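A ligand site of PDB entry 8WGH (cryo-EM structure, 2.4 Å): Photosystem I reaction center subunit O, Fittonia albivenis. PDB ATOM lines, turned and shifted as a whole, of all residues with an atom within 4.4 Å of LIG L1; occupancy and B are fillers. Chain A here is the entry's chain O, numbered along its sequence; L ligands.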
ATOM      1  N   LEU A  61      -5.930  18.211 -34.216  1.00  0.00           N
ATOM      2  CA  LEU A  61      -6.201  19.290 -33.289  1.00  0.00           C
ATOM      3  C   LEU A  61      -4.974  19.741 -32.504  1.00  0.00           C
ATOM      4  O   LEU A  61      -4.945  20.880 -32.042  1.00  0.00           O
ATOM      5  CB  LEU A  61      -7.299  18.861 -32.303  1.00  0.00           C
ATOM      6  CG  LEU A  61      -8.565  19.707 -32.218  1.00  0.00           C
ATOM      7  CD1 LEU A  61      -8.725  20.645 -33.405  1.00  0.00           C
ATOM      8  CD2 LEU A  61      -9.752  18.778 -32.120  1.00  0.00           C
ATOM      9  N   ARG A  62      -3.960  18.875 -32.378  1.00  0.00           N
ATOM     10  CA  ARG A  62      -2.801  19.116 -31.516  1.00  0.00           C
ATOM     11  C   ARG A  62      -3.269  19.471 -30.102  1.00  0.00           C
ATOM     12  O   ARG A  62      -2.954  20.533 -29.569  1.00  0.00           O
ATOM     13  CB  ARG A  62      -1.896  20.194 -32.101  1.00  0.00           C
ATOM     14  CG  ARG A  62      -1.570  19.982 -33.565  1.00  0.00           C
ATOM     15  CD  ARG A  62      -0.602  21.039 -34.065  1.00  0.00           C
ATOM     16  NE  ARG A  62      -1.275  22.289 -34.380  1.00  0.00           N
ATOM     17  CZ  ARG A  62      -0.650  23.399 -34.744  1.00  0.00           C
ATOM     18  NH1 ARG A  62       0.664  23.452 -34.851  1.00  0.00           N
ATOM     19  NH2 ARG A  62      -1.374  24.480 -35.012  1.00  0.00           N
ATOM     20  N   THR A  63      -4.021  18.555 -29.502  1.00  0.00           N
ATOM     21  CA  THR A  63      -4.699  18.818 -28.243  1.00  0.00           C
ATOM     22  C   THR A  63      -3.719  19.177 -27.139  1.00  0.00           C
ATOM     23  O   THR A  63      -2.653  18.571 -27.015  1.00  0.00           O
ATOM     24  CB  THR A  63      -5.520  17.591 -27.822  1.00  0.00           C
ATOM     25  OG1 THR A  63      -4.707  16.706 -27.044  1.00  0.00           O
ATOM     26  CG2 THR A  63      -6.033  16.851 -29.048  1.00  0.00           C
ATOM     27  N   ASP A  64      -4.083  20.187 -26.353  1.00  0.00           N
ATOM     28  CA  ASP A  64      -3.252  20.659 -25.255  1.00  0.00           C
ATOM     29  C   ASP A  64      -3.806  20.324 -23.879  1.00  0.00           C
ATOM     30  O   ASP A  64      -3.025  20.058 -22.968  1.00  0.00           O
ATOM     31  CB  ASP A  64      -3.065  22.179 -25.368  1.00  0.00           C
ATOM     32  CG  ASP A  64      -1.808  22.659 -24.671  1.00  0.00           C
ATOM     33  OD1 ASP A  64      -0.982  21.808 -24.275  1.00  0.00           O
ATOM     34  OD2 ASP A  64      -1.632  23.884 -24.538  1.00  0.00           O
ATOM     35  N   VAL A  67      -5.696  24.413 -22.833  1.00  0.00           N
ATOM     36  CA  VAL A  67      -6.596  25.356 -23.476  1.00  0.00           C
ATOM     37  C   VAL A  67      -8.017  25.233 -22.951  1.00  0.00           C
ATOM     38  O   VAL A  67      -8.672  26.251 -22.714  1.00  0.00           O
ATOM     39  CB  VAL A  67      -6.561  25.179 -25.001  1.00  0.00           C
ATOM     40  CG1 VAL A  67      -7.773  25.823 -25.656  1.00  0.00           C
ATOM     41  CG2 VAL A  67      -5.268  25.738 -25.576  1.00  0.00           C
ATOM     42  N   ILE A  68      -8.500  24.008 -22.746  1.00  0.00           N
ATOM     43  CA  ILE A  68      -9.861  23.831 -22.238  1.00  0.00           C
ATOM     44  C   ILE A  68     -10.029  24.488 -20.878  1.00  0.00           C
ATOM     45  O   ILE A  68     -10.955  25.272 -20.673  1.00  0.00           O
ATOM     46  CB  ILE A  68     -10.221  22.331 -22.175  1.00  0.00           C
ATOM     47  CG1 ILE A  68     -10.281  21.732 -23.574  1.00  0.00           C
ATOM     48  CG2 ILE A  68     -11.540  22.128 -21.445  1.00  0.00           C
ATOM     49  CD1 ILE A  68      -9.426  20.508 -23.755  1.00  0.00           C
ATOM     50  N   ILE A  97     -31.460  26.982 -15.253  1.00  0.00           N
ATOM     51  CA  ILE A  97     -31.378  25.555 -15.549  1.00  0.00           C
ATOM     52  C   ILE A  97     -32.340  24.762 -14.659  1.00  0.00           C
ATOM     53  O   ILE A  97     -33.074  23.879 -15.126  1.00  0.00           O
ATOM     54  CB  ILE A  97     -29.938  25.044 -15.419  1.00  0.00           C
ATOM     55  CG1 ILE A  97     -29.091  25.501 -16.608  1.00  0.00           C
ATOM     56  CG2 ILE A  97     -29.900  23.538 -15.305  1.00  0.00           C
ATOM     57  CD1 ILE A  97     -27.626  25.676 -16.291  1.00  0.00           C
ATOM     58  N   GLU A 100     -36.340  24.567 -15.171  1.00  0.00           N
ATOM     59  CA  GLU A 100     -36.670  23.742 -16.320  1.00  0.00           C
ATOM     60  C   GLU A 100     -36.580  22.266 -15.991  1.00  0.00           C
ATOM     61  O   GLU A 100     -37.428  21.474 -16.430  1.00  0.00           O
ATOM     62  CB  GLU A 100     -35.759  24.076 -17.505  1.00  0.00           C
ATOM     63  CG  GLU A 100     -35.721  25.553 -17.855  1.00  0.00           C
ATOM     64  CD  GLU A 100     -37.090  26.134 -18.145  1.00  0.00           C
ATOM     65  OE1 GLU A 100     -37.930  25.422 -18.737  1.00  0.00           O
ATOM     66  OE2 GLU A 100     -37.338  27.299 -17.778  1.00  0.00           O
ATOM     67  N   LEU A 101     -35.577  21.865 -15.211  1.00  0.00           N
ATOM     68  CA  LEU A 101     -35.481  20.484 -14.741  1.00  0.00           C
ATOM     69  C   LEU A 101     -36.590  20.120 -13.782  1.00  0.00           C
ATOM     70  O   LEU A 101     -36.870  18.925 -13.602  1.00  0.00           O
ATOM     71  CB  LEU A 101     -34.127  20.262 -14.060  1.00  0.00           C
ATOM     72  CG  LEU A 101     -32.983  19.778 -14.952  1.00  0.00           C
ATOM     73  CD1 LEU A 101     -31.793  19.352 -14.114  1.00  0.00           C
ATOM     74  CD2 LEU A 101     -33.457  18.643 -15.836  1.00  0.00           C
ATOM     75  N   PHE A 104     -39.373  17.939 -15.593  1.00  0.00           N
ATOM     76  CA  PHE A 104     -38.922  16.876 -16.474  1.00  0.00           C
ATOM     77  C   PHE A 104     -40.052  15.872 -16.693  1.00  0.00           C
ATOM     78  O   PHE A 104     -40.842  15.625 -15.777  1.00  0.00           O
ATOM     79  CB  PHE A 104     -37.704  16.184 -15.873  1.00  0.00           C
ATOM     80  CG  PHE A 104     -36.910  15.369 -16.856  1.00  0.00           C
ATOM     81  CD1 PHE A 104     -36.132  15.987 -17.813  1.00  0.00           C
ATOM     82  CD2 PHE A 104     -36.953  13.984 -16.818  1.00  0.00           C
ATOM     83  CE1 PHE A 104     -35.396  15.241 -18.719  1.00  0.00           C
ATOM     84  CE2 PHE A 104     -36.226  13.240 -17.720  1.00  0.00           C
ATOM     85  CZ  PHE A 104     -35.448  13.858 -18.677  1.00  0.00           C
ATOM     86  N   THR A 106     -40.800  17.270 -19.757  1.00  0.00           N
ATOM     87  CA  THR A 106     -41.256  18.286 -20.689  1.00  0.00           C
ATOM     88  C   THR A 106     -40.193  19.364 -20.868  1.00  0.00           C
ATOM     89  O   THR A 106     -39.560  19.813 -19.914  1.00  0.00           O
ATOM     90  CB  THR A 106     -42.565  18.919 -20.195  1.00  0.00           C
ATOM     91  OG1 THR A 106     -42.371  19.441 -18.878  1.00  0.00           O
ATOM     92  CG2 THR A 106     -43.679  17.894 -20.178  1.00  0.00           C
ATOM     93  N   GLY A 107     -39.989  19.762 -22.126  1.00  0.00           N
ATOM     94  CA  GLY A 107     -38.972  20.736 -22.454  1.00  0.00           C
ATOM     95  C   GLY A 107     -39.385  22.152 -22.099  1.00  0.00           C
ATOM     96  O   GLY A 107     -40.550  22.427 -21.800  1.00  0.00           O
ATOM     97  N   PRO A 108     -38.414  23.064 -22.115  1.00  0.00           N
ATOM     98  CA  PRO A 108     -38.734  24.473 -21.822  1.00  0.00           C
ATOM     99  C   PRO A 108     -39.714  25.038 -22.830  1.00  0.00           C
ATOM    100  O   PRO A 108     -39.721  24.682 -24.003  1.00  0.00           O
ATOM    101  CB  PRO A 108     -37.374  25.178 -21.904  1.00  0.00           C
ATOM    102  CG  PRO A 108     -36.338  24.123 -21.954  1.00  0.00           C
ATOM    103  CD  PRO A 108     -36.974  22.794 -22.183  1.00  0.00           C
ATOM    104  N   PHE A 114     -34.834  30.591 -20.541  1.00  0.00           N
ATOM    105  CA  PHE A 114     -33.696  29.669 -20.591  1.00  0.00           C
ATOM    106  C   PHE A 114     -32.915  29.824 -21.894  1.00  0.00           C
ATOM    107  O   PHE A 114     -31.686  29.789 -21.901  1.00  0.00           O
ATOM    108  CB  PHE A 114     -34.215  28.243 -20.426  1.00  0.00           C
ATOM    109  CG  PHE A 114     -33.216  27.172 -20.799  1.00  0.00           C
ATOM    110  CD1 PHE A 114     -32.266  26.744 -19.887  1.00  0.00           C
ATOM    111  CD2 PHE A 114     -33.252  26.581 -22.047  1.00  0.00           C
ATOM    112  CE1 PHE A 114     -31.362  25.772 -20.223  1.00  0.00           C
ATOM    113  CE2 PHE A 114     -32.340  25.607 -22.387  1.00  0.00           C
ATOM    114  CZ  PHE A 114     -31.399  25.189 -21.477  1.00  0.00           C
ATOM    115  N   LEU A 129     -12.918  29.792 -25.890  1.00  0.00           N
ATOM    116  CA  LEU A 129     -12.183  28.555 -26.178  1.00  0.00           C
ATOM    117  C   LEU A 129     -11.461  28.643 -27.517  1.00  0.00           C
ATOM    118  O   LEU A 129     -10.279  28.314 -27.629  1.00  0.00           O
ATOM    119  CB  LEU A 129     -13.145  27.373 -26.152  1.00  0.00           C
ATOM    120  CG  LEU A 129     -13.440  26.746 -24.786  1.00  0.00           C
ATOM    121  CD1 LEU A 129     -14.458  25.642 -24.922  1.00  0.00           C
ATOM    122  CD2 LEU A 129     -12.163  26.226 -24.155  1.00  0.00           C
ATOM    123  N   GLN A 133      -7.374  28.712 -28.087  1.00  0.00           N
ATOM    124  CA  GLN A 133      -6.686  27.727 -28.908  1.00  0.00           C
ATOM    125  C   GLN A 133      -5.895  28.401 -30.018  1.00  0.00           C
ATOM    126  O   GLN A 133      -4.734  28.040 -30.263  1.00  0.00           O
ATOM    127  CB  GLN A 133      -7.706  26.734 -29.489  1.00  0.00           C
ATOM    128  CG  GLN A 133      -7.208  25.963 -30.698  1.00  0.00           C
ATOM    129  CD  GLN A 133      -6.448  24.712 -30.328  1.00  0.00           C
ATOM    130  OE1 GLN A 133      -6.250  24.416 -29.148  1.00  0.00           O
ATOM    131  NE2 GLN A 133      -6.011  23.962 -31.334  1.00  0.00           N
HETATM  132  C1  LIG L   1     -32.565  21.090 -19.704  1.00  0.00           C
HETATM  133  C2  LIG L   1     -34.083  20.936 -19.911  1.00  0.00           C
HETATM  134  C3  LIG L   1     -34.671  19.560 -19.660  1.00  0.00           C
HETATM  135  C4  LIG L   1     -33.749  18.474 -20.169  1.00  0.00           C
HETATM  136  C5  LIG L   1     -32.425  18.613 -19.449  1.00  0.00           C
HETATM  137  C6  LIG L   1     -31.843  19.802 -19.366  1.00  0.00           C
HETATM  138  C7  LIG L   1     -30.431  19.899 -18.939  1.00  0.00           C
HETATM  139  C8  LIG L   1     -29.463  19.613 -19.796  1.00  0.00           C
HETATM  140  C9  LIG L   1     -28.030  19.703 -19.437  1.00  0.00           C
HETATM  141  C10 LIG L   1     -27.130  19.499 -20.394  1.00  0.00           C
HETATM  142  C11 LIG L   1     -25.689  19.594 -20.174  1.00  0.00           C
HETATM  143  C12 LIG L   1     -24.925  19.503 -21.264  1.00  0.00           C
HETATM  144  C13 LIG L   1     -23.461  19.593 -21.216  1.00  0.00           C
HETATM  145  C14 LIG L   1     -22.786  19.453 -22.363  1.00  0.00           C
HETATM  146  C15 LIG L   1     -21.334  19.571 -22.415  1.00  0.00           C
HETATM  147  C16 LIG L   1     -32.336  22.064 -18.552  1.00  0.00           C
HETATM  148  C17 LIG L   1     -31.961  21.674 -20.972  1.00  0.00           C
HETATM  149  C18 LIG L   1     -31.817  17.390 -18.833  1.00  0.00           C
HETATM  150  C19 LIG L   1     -27.606  20.022 -18.031  1.00  0.00           C
HETATM  151  C20 LIG L   1     -22.750  19.866 -19.925  1.00  0.00           C
HETATM  152  O1  LIG L   1     -35.922  19.462 -20.348  1.00  0.00           O
HETATM  153  C21 LIG L   1     -10.142  22.261 -27.878  1.00  0.00           C
HETATM  154  C22 LIG L   1      -8.647  22.517 -27.805  1.00  0.00           C
HETATM  155  C23 LIG L   1      -7.826  21.444 -28.510  1.00  0.00           C
HETATM  156  C24 LIG L   1      -8.319  20.059 -28.163  1.00  0.00           C
HETATM  157  C25 LIG L   1      -9.600  19.813 -27.863  1.00  0.00           C
HETATM  158  C26 LIG L   1     -10.485  20.890 -27.302  1.00  0.00           C
HETATM  159  C27 LIG L   1     -11.942  20.592 -27.588  1.00  0.00           C
HETATM  160  C28 LIG L   1     -12.746  20.272 -26.579  1.00  0.00           C
HETATM  161  C29 LIG L   1     -14.174  19.996 -26.801  1.00  0.00           C
HETATM  162  C30 LIG L   1     -14.959  19.798 -25.723  1.00  0.00           C
HETATM  163  C31 LIG L   1     -16.392  19.544 -25.857  1.00  0.00           C
HETATM  164  C32 LIG L   1     -17.110  19.545 -24.747  1.00  0.00           C
HETATM  165  C33 LIG L   1     -18.569  19.338 -24.754  1.00  0.00           C
HETATM  166  C34 LIG L   1     -19.252  19.527 -23.623  1.00  0.00           C
HETATM  167  C35 LIG L   1     -20.698  19.376 -23.566  1.00  0.00           C
HETATM  168  C36 LIG L   1     -10.628  22.364 -29.313  1.00  0.00           C
HETATM  169  C37 LIG L   1     -10.849  23.324 -27.044  1.00  0.00           C
HETATM  170  C38 LIG L   1     -10.145  18.425 -28.068  1.00  0.00           C
HETATM  171  C39 LIG L   1     -14.744  19.950 -28.192  1.00  0.00           C
HETATM  172  C40 LIG L   1     -19.271  18.940 -26.015  1.00  0.00           C
HETATM  173  O2  LIG L   1      -6.455  21.561 -28.083  1.00  0.00           O
HETATM  174 MG1  LG2 L   2     -23.168  23.048 -22.393  1.00  0.00          MG
HETATM  175  C1  LG2 L   2     -26.189  22.759 -24.090  1.00  0.00           C
HETATM  176  C2  LG2 L   2     -21.500  22.647 -25.317  1.00  0.00           C
HETATM  177  C3  LG2 L   2     -20.224  23.470 -20.684  1.00  0.00           C
HETATM  178  C4  LG2 L   2     -24.971  23.480 -19.365  1.00  0.00           C
HETATM  179  N1  LG2 L   2     -23.778  22.747 -24.372  1.00  0.00           N
HETATM  180  C5  LG2 L   2     -25.078  22.668 -24.879  1.00  0.00           C
HETATM  181  C6  LG2 L   2     -25.068  22.460 -26.393  1.00  0.00           C
HETATM  182  C7  LG2 L   2     -23.569  22.288 -26.722  1.00  0.00           C
HETATM  183  C8  LG2 L   2     -22.874  22.599 -25.390  1.00  0.00           C
HETATM  184  C9  LG2 L   2     -23.206  20.887 -27.153  1.00  0.00           C
HETATM  185  C10 LG2 L   2     -25.678  23.643 -27.123  1.00  0.00           C
HETATM  186  C11 LG2 L   2     -24.655  24.737 -27.344  1.00  0.00           C
HETATM  187  C12 LG2 L   2     -25.329  26.025 -27.745  1.00  0.00           C
HETATM  188  O1  LG2 L   2     -25.057  26.554 -28.804  1.00  0.00           O
HETATM  189  O2  LG2 L   2     -26.278  26.659 -26.861  1.00  0.00           O
HETATM  190  N2  LG2 L   2     -21.229  23.052 -22.912  1.00  0.00           N
HETATM  191  C13 LG2 L   2     -20.744  22.891 -24.167  1.00  0.00           C
HETATM  192  C14 LG2 L   2     -19.257  23.000 -24.149  1.00  0.00           C
HETATM  193  C15 LG2 L   2     -18.885  23.232 -22.844  1.00  0.00           C
HETATM  194  C16 LG2 L   2     -20.134  23.266 -22.026  1.00  0.00           C
HETATM  195  C17 LG2 L   2     -18.328  22.860 -25.321  1.00  0.00           C
HETATM  196  C18 LG2 L   2     -17.492  23.383 -22.370  1.00  0.00           C
HETATM  197  C19 LG2 L   2     -17.206  23.370 -21.091  1.00  0.00           C
HETATM  198  N3  LG2 L   2     -22.760  23.454 -20.405  1.00  0.00           N
HETATM  199  C20 LG2 L   2     -21.420  23.530 -19.909  1.00  0.00           C
HETATM  200  C21 LG2 L   2     -21.457  23.754 -18.475  1.00  0.00           C
HETATM  201  C22 LG2 L   2     -22.796  23.769 -18.100  1.00  0.00           C
HETATM  202  C23 LG2 L   2     -23.569  23.543 -19.311  1.00  0.00           C
HETATM  203  C24 LG2 L   2     -20.287  23.963 -17.554  1.00  0.00           C
HETATM  204  C25 LG2 L   2     -23.364  23.972 -16.716  1.00  0.00           C
HETATM  205  C26 LG2 L   2     -24.359  22.874 -16.398  1.00  0.00           C
HETATM  206  N4  LG2 L   2     -25.098  23.100 -21.793  1.00  0.00           N
HETATM  207  C27 LG2 L   2     -25.707  23.274 -20.516  1.00  0.00           C
HETATM  208  C28 LG2 L   2     -27.172  23.202 -20.663  1.00  0.00           C
HETATM  209  C29 LG2 L   2     -27.410  22.984 -22.005  1.00  0.00           C
HETATM  210  C30 LG2 L   2     -26.094  22.930 -22.667  1.00  0.00           C
HETATM  211  C31 LG2 L   2     -28.354  23.279 -19.739  1.00  0.00           C
HETATM  212  C32 LG2 L   2     -28.413  22.803 -23.039  1.00  0.00           C
HETATM  213  O3  LG2 L   2     -29.675  22.781 -22.894  1.00  0.00           O
HETATM  214  C33 LG2 L   2     -27.663  22.637 -24.381  1.00  0.00           C
HETATM  215  C34 LG2 L   2     -27.918  21.328 -25.058  1.00  0.00           C
HETATM  216  O4  LG2 L   2     -28.791  21.198 -25.893  1.00  0.00           O
HETATM  217  O5  LG2 L   2     -27.126  20.157 -24.772  1.00  0.00           O
HETATM  218  C35 LG2 L   2     -27.424  18.951 -25.468  1.00  0.00           C
HETATM  219 MG1  LG3 L   3     -36.285  17.101 -24.433  1.00  0.00          MG
HETATM  220  C1  LG3 L   3     -39.496  17.574 -25.687  1.00  0.00           C
HETATM  221  C2  LG3 L   3     -37.047  13.864 -23.734  1.00  0.00           C
HETATM  222  C3  LG3 L   3     -33.076  16.664 -23.306  1.00  0.00           C
HETATM  223  C4  LG3 L   3     -35.530  20.469 -25.226  1.00  0.00           C
HETATM  224  N1  LG3 L   3     -38.000  15.934 -24.671  1.00  0.00           N
HETATM  225  C5  LG3 L   3     -39.235  16.316 -25.226  1.00  0.00           C
HETATM  226  C6  LG3 L   3     -40.218  15.141 -25.220  1.00  0.00           C
HETATM  227  C7  LG3 L   3     -39.427  14.006 -24.541  1.00  0.00           C
HETATM  228  C8  LG3 L   3     -38.052  14.621 -24.291  1.00  0.00           C
HETATM  229  C9  LG3 L   3     -40.085  13.557 -23.263  1.00  0.00           C
HETATM  230  C10 LG3 L   3     -40.547  14.745 -26.651  1.00  0.00           C
HETATM  231  C11 LG3 L   3     -41.938  14.166 -26.772  1.00  0.00           C
HETATM  232  C12 LG3 L   3     -42.357  14.176 -28.212  1.00  0.00           C
HETATM  233  O1  LG3 L   3     -41.699  13.862 -29.202  1.00  0.00           O
HETATM  234  O2  LG3 L   3     -43.649  14.588 -28.389  1.00  0.00           O
HETATM  235  N2  LG3 L   3     -35.241  15.550 -23.694  1.00  0.00           N
HETATM  236  C13 LG3 L   3     -35.744  14.311 -23.435  1.00  0.00           C
HETATM  237  C14 LG3 L   3     -34.708  13.475 -22.783  1.00  0.00           C
HETATM  238  C15 LG3 L   3     -33.578  14.258 -22.657  1.00  0.00           C
HETATM  239  C16 LG3 L   3     -33.903  15.592 -23.230  1.00  0.00           C
HETATM  240  C17 LG3 L   3     -34.933  12.092 -22.370  1.00  0.00           C
HETATM  241  C18 LG3 L   3     -32.302  13.936 -22.075  1.00  0.00           C
HETATM  242  C19 LG3 L   3     -31.124  13.988 -22.718  1.00  0.00           C
HETATM  243  N3  LG3 L   3     -34.619  18.351 -24.280  1.00  0.00           N
HETATM  244  C20 LG3 L   3     -33.399  17.959 -23.793  1.00  0.00           C
HETATM  245  C21 LG3 L   3     -32.463  19.077 -23.838  1.00  0.00           C
HETATM  246  C22 LG3 L   3     -33.152  20.154 -24.388  1.00  0.00           C
HETATM  247  C23 LG3 L   3     -34.506  19.691 -24.666  1.00  0.00           C
HETATM  248  C24 LG3 L   3     -31.069  19.015 -23.393  1.00  0.00           C
HETATM  249  C25 LG3 L   3     -32.640  21.509 -24.640  1.00  0.00           C
HETATM  250  C26 LG3 L   3     -32.225  21.699 -26.080  1.00  0.00           C
HETATM  251  N4  LG3 L   3     -37.245  18.711 -25.190  1.00  0.00           N
HETATM  252  C27 LG3 L   3     -36.811  20.027 -25.486  1.00  0.00           C
HETATM  253  C28 LG3 L   3     -37.937  20.794 -26.080  1.00  0.00           C
HETATM  254  C29 LG3 L   3     -38.996  19.898 -26.171  1.00  0.00           C
HETATM  255  C30 LG3 L   3     -38.509  18.614 -25.623  1.00  0.00           C
HETATM  256  C31 LG3 L   3     -37.878  22.189 -26.483  1.00  0.00           C
HETATM  257  C32 LG3 L   3     -40.378  19.706 -26.563  1.00  0.00           C
HETATM  258  O3  LG3 L   3     -41.184  20.533 -26.997  1.00  0.00           O
HETATM  259  C33 LG3 L   3     -40.724  18.206 -26.321  1.00  0.00           C
HETATM  260  C34 LG3 L   3     -41.978  18.042 -25.509  1.00  0.00           C
HETATM  261  O4  LG3 L   3     -43.137  18.241 -25.880  1.00  0.00           O
HETATM  262  O5  LG3 L   3     -41.786  17.605 -24.232  1.00  0.00           O
HETATM  263  C35 LG3 L   3     -42.821  16.811 -23.652  1.00  0.00           C
HETATM  264 MG1  LG4 L   4      -8.568  29.533 -36.888  1.00  0.00          MG
HETATM  265  C1  LG4 L   4      -7.565  26.613 -35.315  1.00  0.00           C
HETATM  266  C2  LG4 L   4     -11.777  28.394 -36.938  1.00  0.00           C
HETATM  267  C3  LG4 L   4      -9.550  32.541 -38.225  1.00  0.00           C
HETATM  268  C4  LG4 L   4      -5.235  30.710 -36.710  1.00  0.00           C
HETATM  269  N1  LG4 L   4      -9.483  27.765 -36.265  1.00  0.00           N
HETATM  270  C5  LG4 L   4      -8.904  26.673 -35.610  1.00  0.00           C
HETATM  271  C6  LG4 L   4      -9.942  25.590 -35.316  1.00  0.00           C
HETATM  272  C7  LG4 L   4     -11.219  26.123 -35.998  1.00  0.00           C
HETATM  273  C8  LG4 L   4     -10.819  27.531 -36.441  1.00  0.00           C
HETATM  274  C9  LG4 L   4     -11.649  25.264 -37.164  1.00  0.00           C
HETATM  275  C10 LG4 L   4     -10.145  25.436 -33.822  1.00  0.00           C
HETATM  276  C11 LG4 L   4     -11.609  25.376 -33.430  1.00  0.00           C
HETATM  277  C12 LG4 L   4     -11.731  25.316 -31.937  1.00  0.00           C
HETATM  278  O1  LG4 L   4     -11.037  25.860 -31.085  1.00  0.00           O
HETATM  279  O2  LG4 L   4     -12.778  24.535 -31.516  1.00  0.00           O
HETATM  280  N2  LG4 L   4     -10.324  30.318 -37.475  1.00  0.00           N
HETATM  281  C13 LG4 L   4     -11.529  29.699 -37.381  1.00  0.00           C
HETATM  282  C14 LG4 L   4     -12.605  30.643 -37.811  1.00  0.00           C
HETATM  283  C15 LG4 L   4     -11.988  31.814 -38.173  1.00  0.00           C
HETATM  284  C16 LG4 L   4     -10.528  31.624 -37.983  1.00  0.00           C
HETATM  285  C17 LG4 L   4     -14.021  30.283 -37.819  1.00  0.00           C
HETATM  286  C18 LG4 L   4     -12.564  33.030 -38.663  1.00  0.00           C
HETATM  287  C19 LG4 L   4     -12.489  33.445 -39.928  1.00  0.00           C
HETATM  288  N3  LG4 L   4      -7.558  31.279 -37.433  1.00  0.00           N
HETATM  289  C20 LG4 L   4      -8.150  32.379 -37.984  1.00  0.00           C
HETATM  290  C21 LG4 L   4      -7.159  33.412 -38.236  1.00  0.00           C
HETATM  291  C22 LG4 L   4      -5.933  32.917 -37.776  1.00  0.00           C
HETATM  292  C23 LG4 L   4      -6.195  31.566 -37.273  1.00  0.00           C
HETATM  293  C24 LG4 L   4      -7.435  34.712 -38.831  1.00  0.00           C
HETATM  294  C25 LG4 L   4      -4.638  33.606 -37.799  1.00  0.00           C
HETATM  295  C26 LG4 L   4      -4.149  33.990 -36.431  1.00  0.00           C
HETATM  296  N4  LG4 L   4      -6.758  28.835 -36.306  1.00  0.00           N
HETATM  297  C27 LG4 L   4      -5.478  29.432 -36.248  1.00  0.00           C
HETATM  298  C28 LG4 L   4      -4.518  28.483 -35.643  1.00  0.00           C
HETATM  299  C29 LG4 L   4      -5.268  27.373 -35.275  1.00  0.00           C
HETATM  300  C30 LG4 L   4      -6.655  27.659 -35.678  1.00  0.00           C
HETATM  301  C31 LG4 L   4      -3.090  28.734 -35.475  1.00  0.00           C
HETATM  302  C32 LG4 L   4      -5.252  26.056 -34.681  1.00  0.00           C
HETATM  303  O3  LG4 L   4      -4.302  25.385 -34.309  1.00  0.00           O
HETATM  304  C33 LG4 L   4      -6.726  25.563 -34.605  1.00  0.00           C
HETATM  305  C34 LG4 L   4      -6.925  24.198 -35.194  1.00  0.00           C
HETATM  306  O4  LG4 L   4      -7.779  23.364 -34.887  1.00  0.00           O
HETATM  307  O5  LG4 L   4      -6.036  23.875 -36.183  1.00  0.00           O
HETATM  308  C35 LG4 L   4      -5.958  22.504 -36.576  1.00  0.00           C
HETATM  309  C36 LG4 L   4     -13.964  25.235 -31.105  1.00  0.00           C
HETATM  310  C37 LG4 L   4     -14.243  24.838 -29.706  1.00  0.00           C
HETATM  311  C38 LG4 L   4     -15.218  23.970 -29.373  1.00  0.00           C
HETATM  312  C39 LG4 L   4     -15.474  23.587 -27.958  1.00  0.00           C
HETATM  313  C40 LG4 L   4     -16.095  23.357 -30.404  1.00  0.00           C
HETATM  314  C41 LG4 L   4     -17.559  23.373 -30.025  1.00  0.00           C
HETATM  315  C42 LG4 L   4     -18.117  21.969 -29.964  1.00  0.00           C
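The side-chain amide oxygen (OE1) of Gln 133 lies within hydrogen-bond range of an oxygen (O2) of LIG L1, 3.1 Å away. The backbone NH (N) of Asp 64 is in hydrogen-bond range of an oxygen (O2) of LIG L1 (3.2 Å). An oxygen (O3) of LG4 L4 is in hydrogen-bond range of the guanidinium group (NH2) of Arg 62, 3.1 Å away.
The side-chain amide nitrogen (NE2) of Gln 133 lies within hydrogen-bond range of the backbone carbonyl oxygen (O) of Leu 61 (3.3 Å).
O of Arg 62 touches O2 of LIG L1 (3.9 Å). Thr 63 touches LIG L1. Ile 68 touches LIG L1. Ile 97 touches LIG L1 (O to C16, 3.9 Å). Leu 101 touches LIG L1 (CD2 to C18, 3.6 Å). CE1 of Phe 104 touches C4 of LIG L1, 3.9 Å away. Thr 106 touches LIG L1. Gly 107 touches LIG L1 (CA to O1, 3.9 Å). Pro 108 touches LIG L1 (CD to O1, 3.9 Å). CZ of Phe 114 touches C17 of LIG L1, at 3.6 Å. Hydrophobic or aromatic side chains within 4 Å of LIG L1: Ile 68, Leu 101, Phe 104, Pro 108 and Phe 114. The nearest printed residue that does not touch LIG L1 is Val 67 (4.04 Å).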
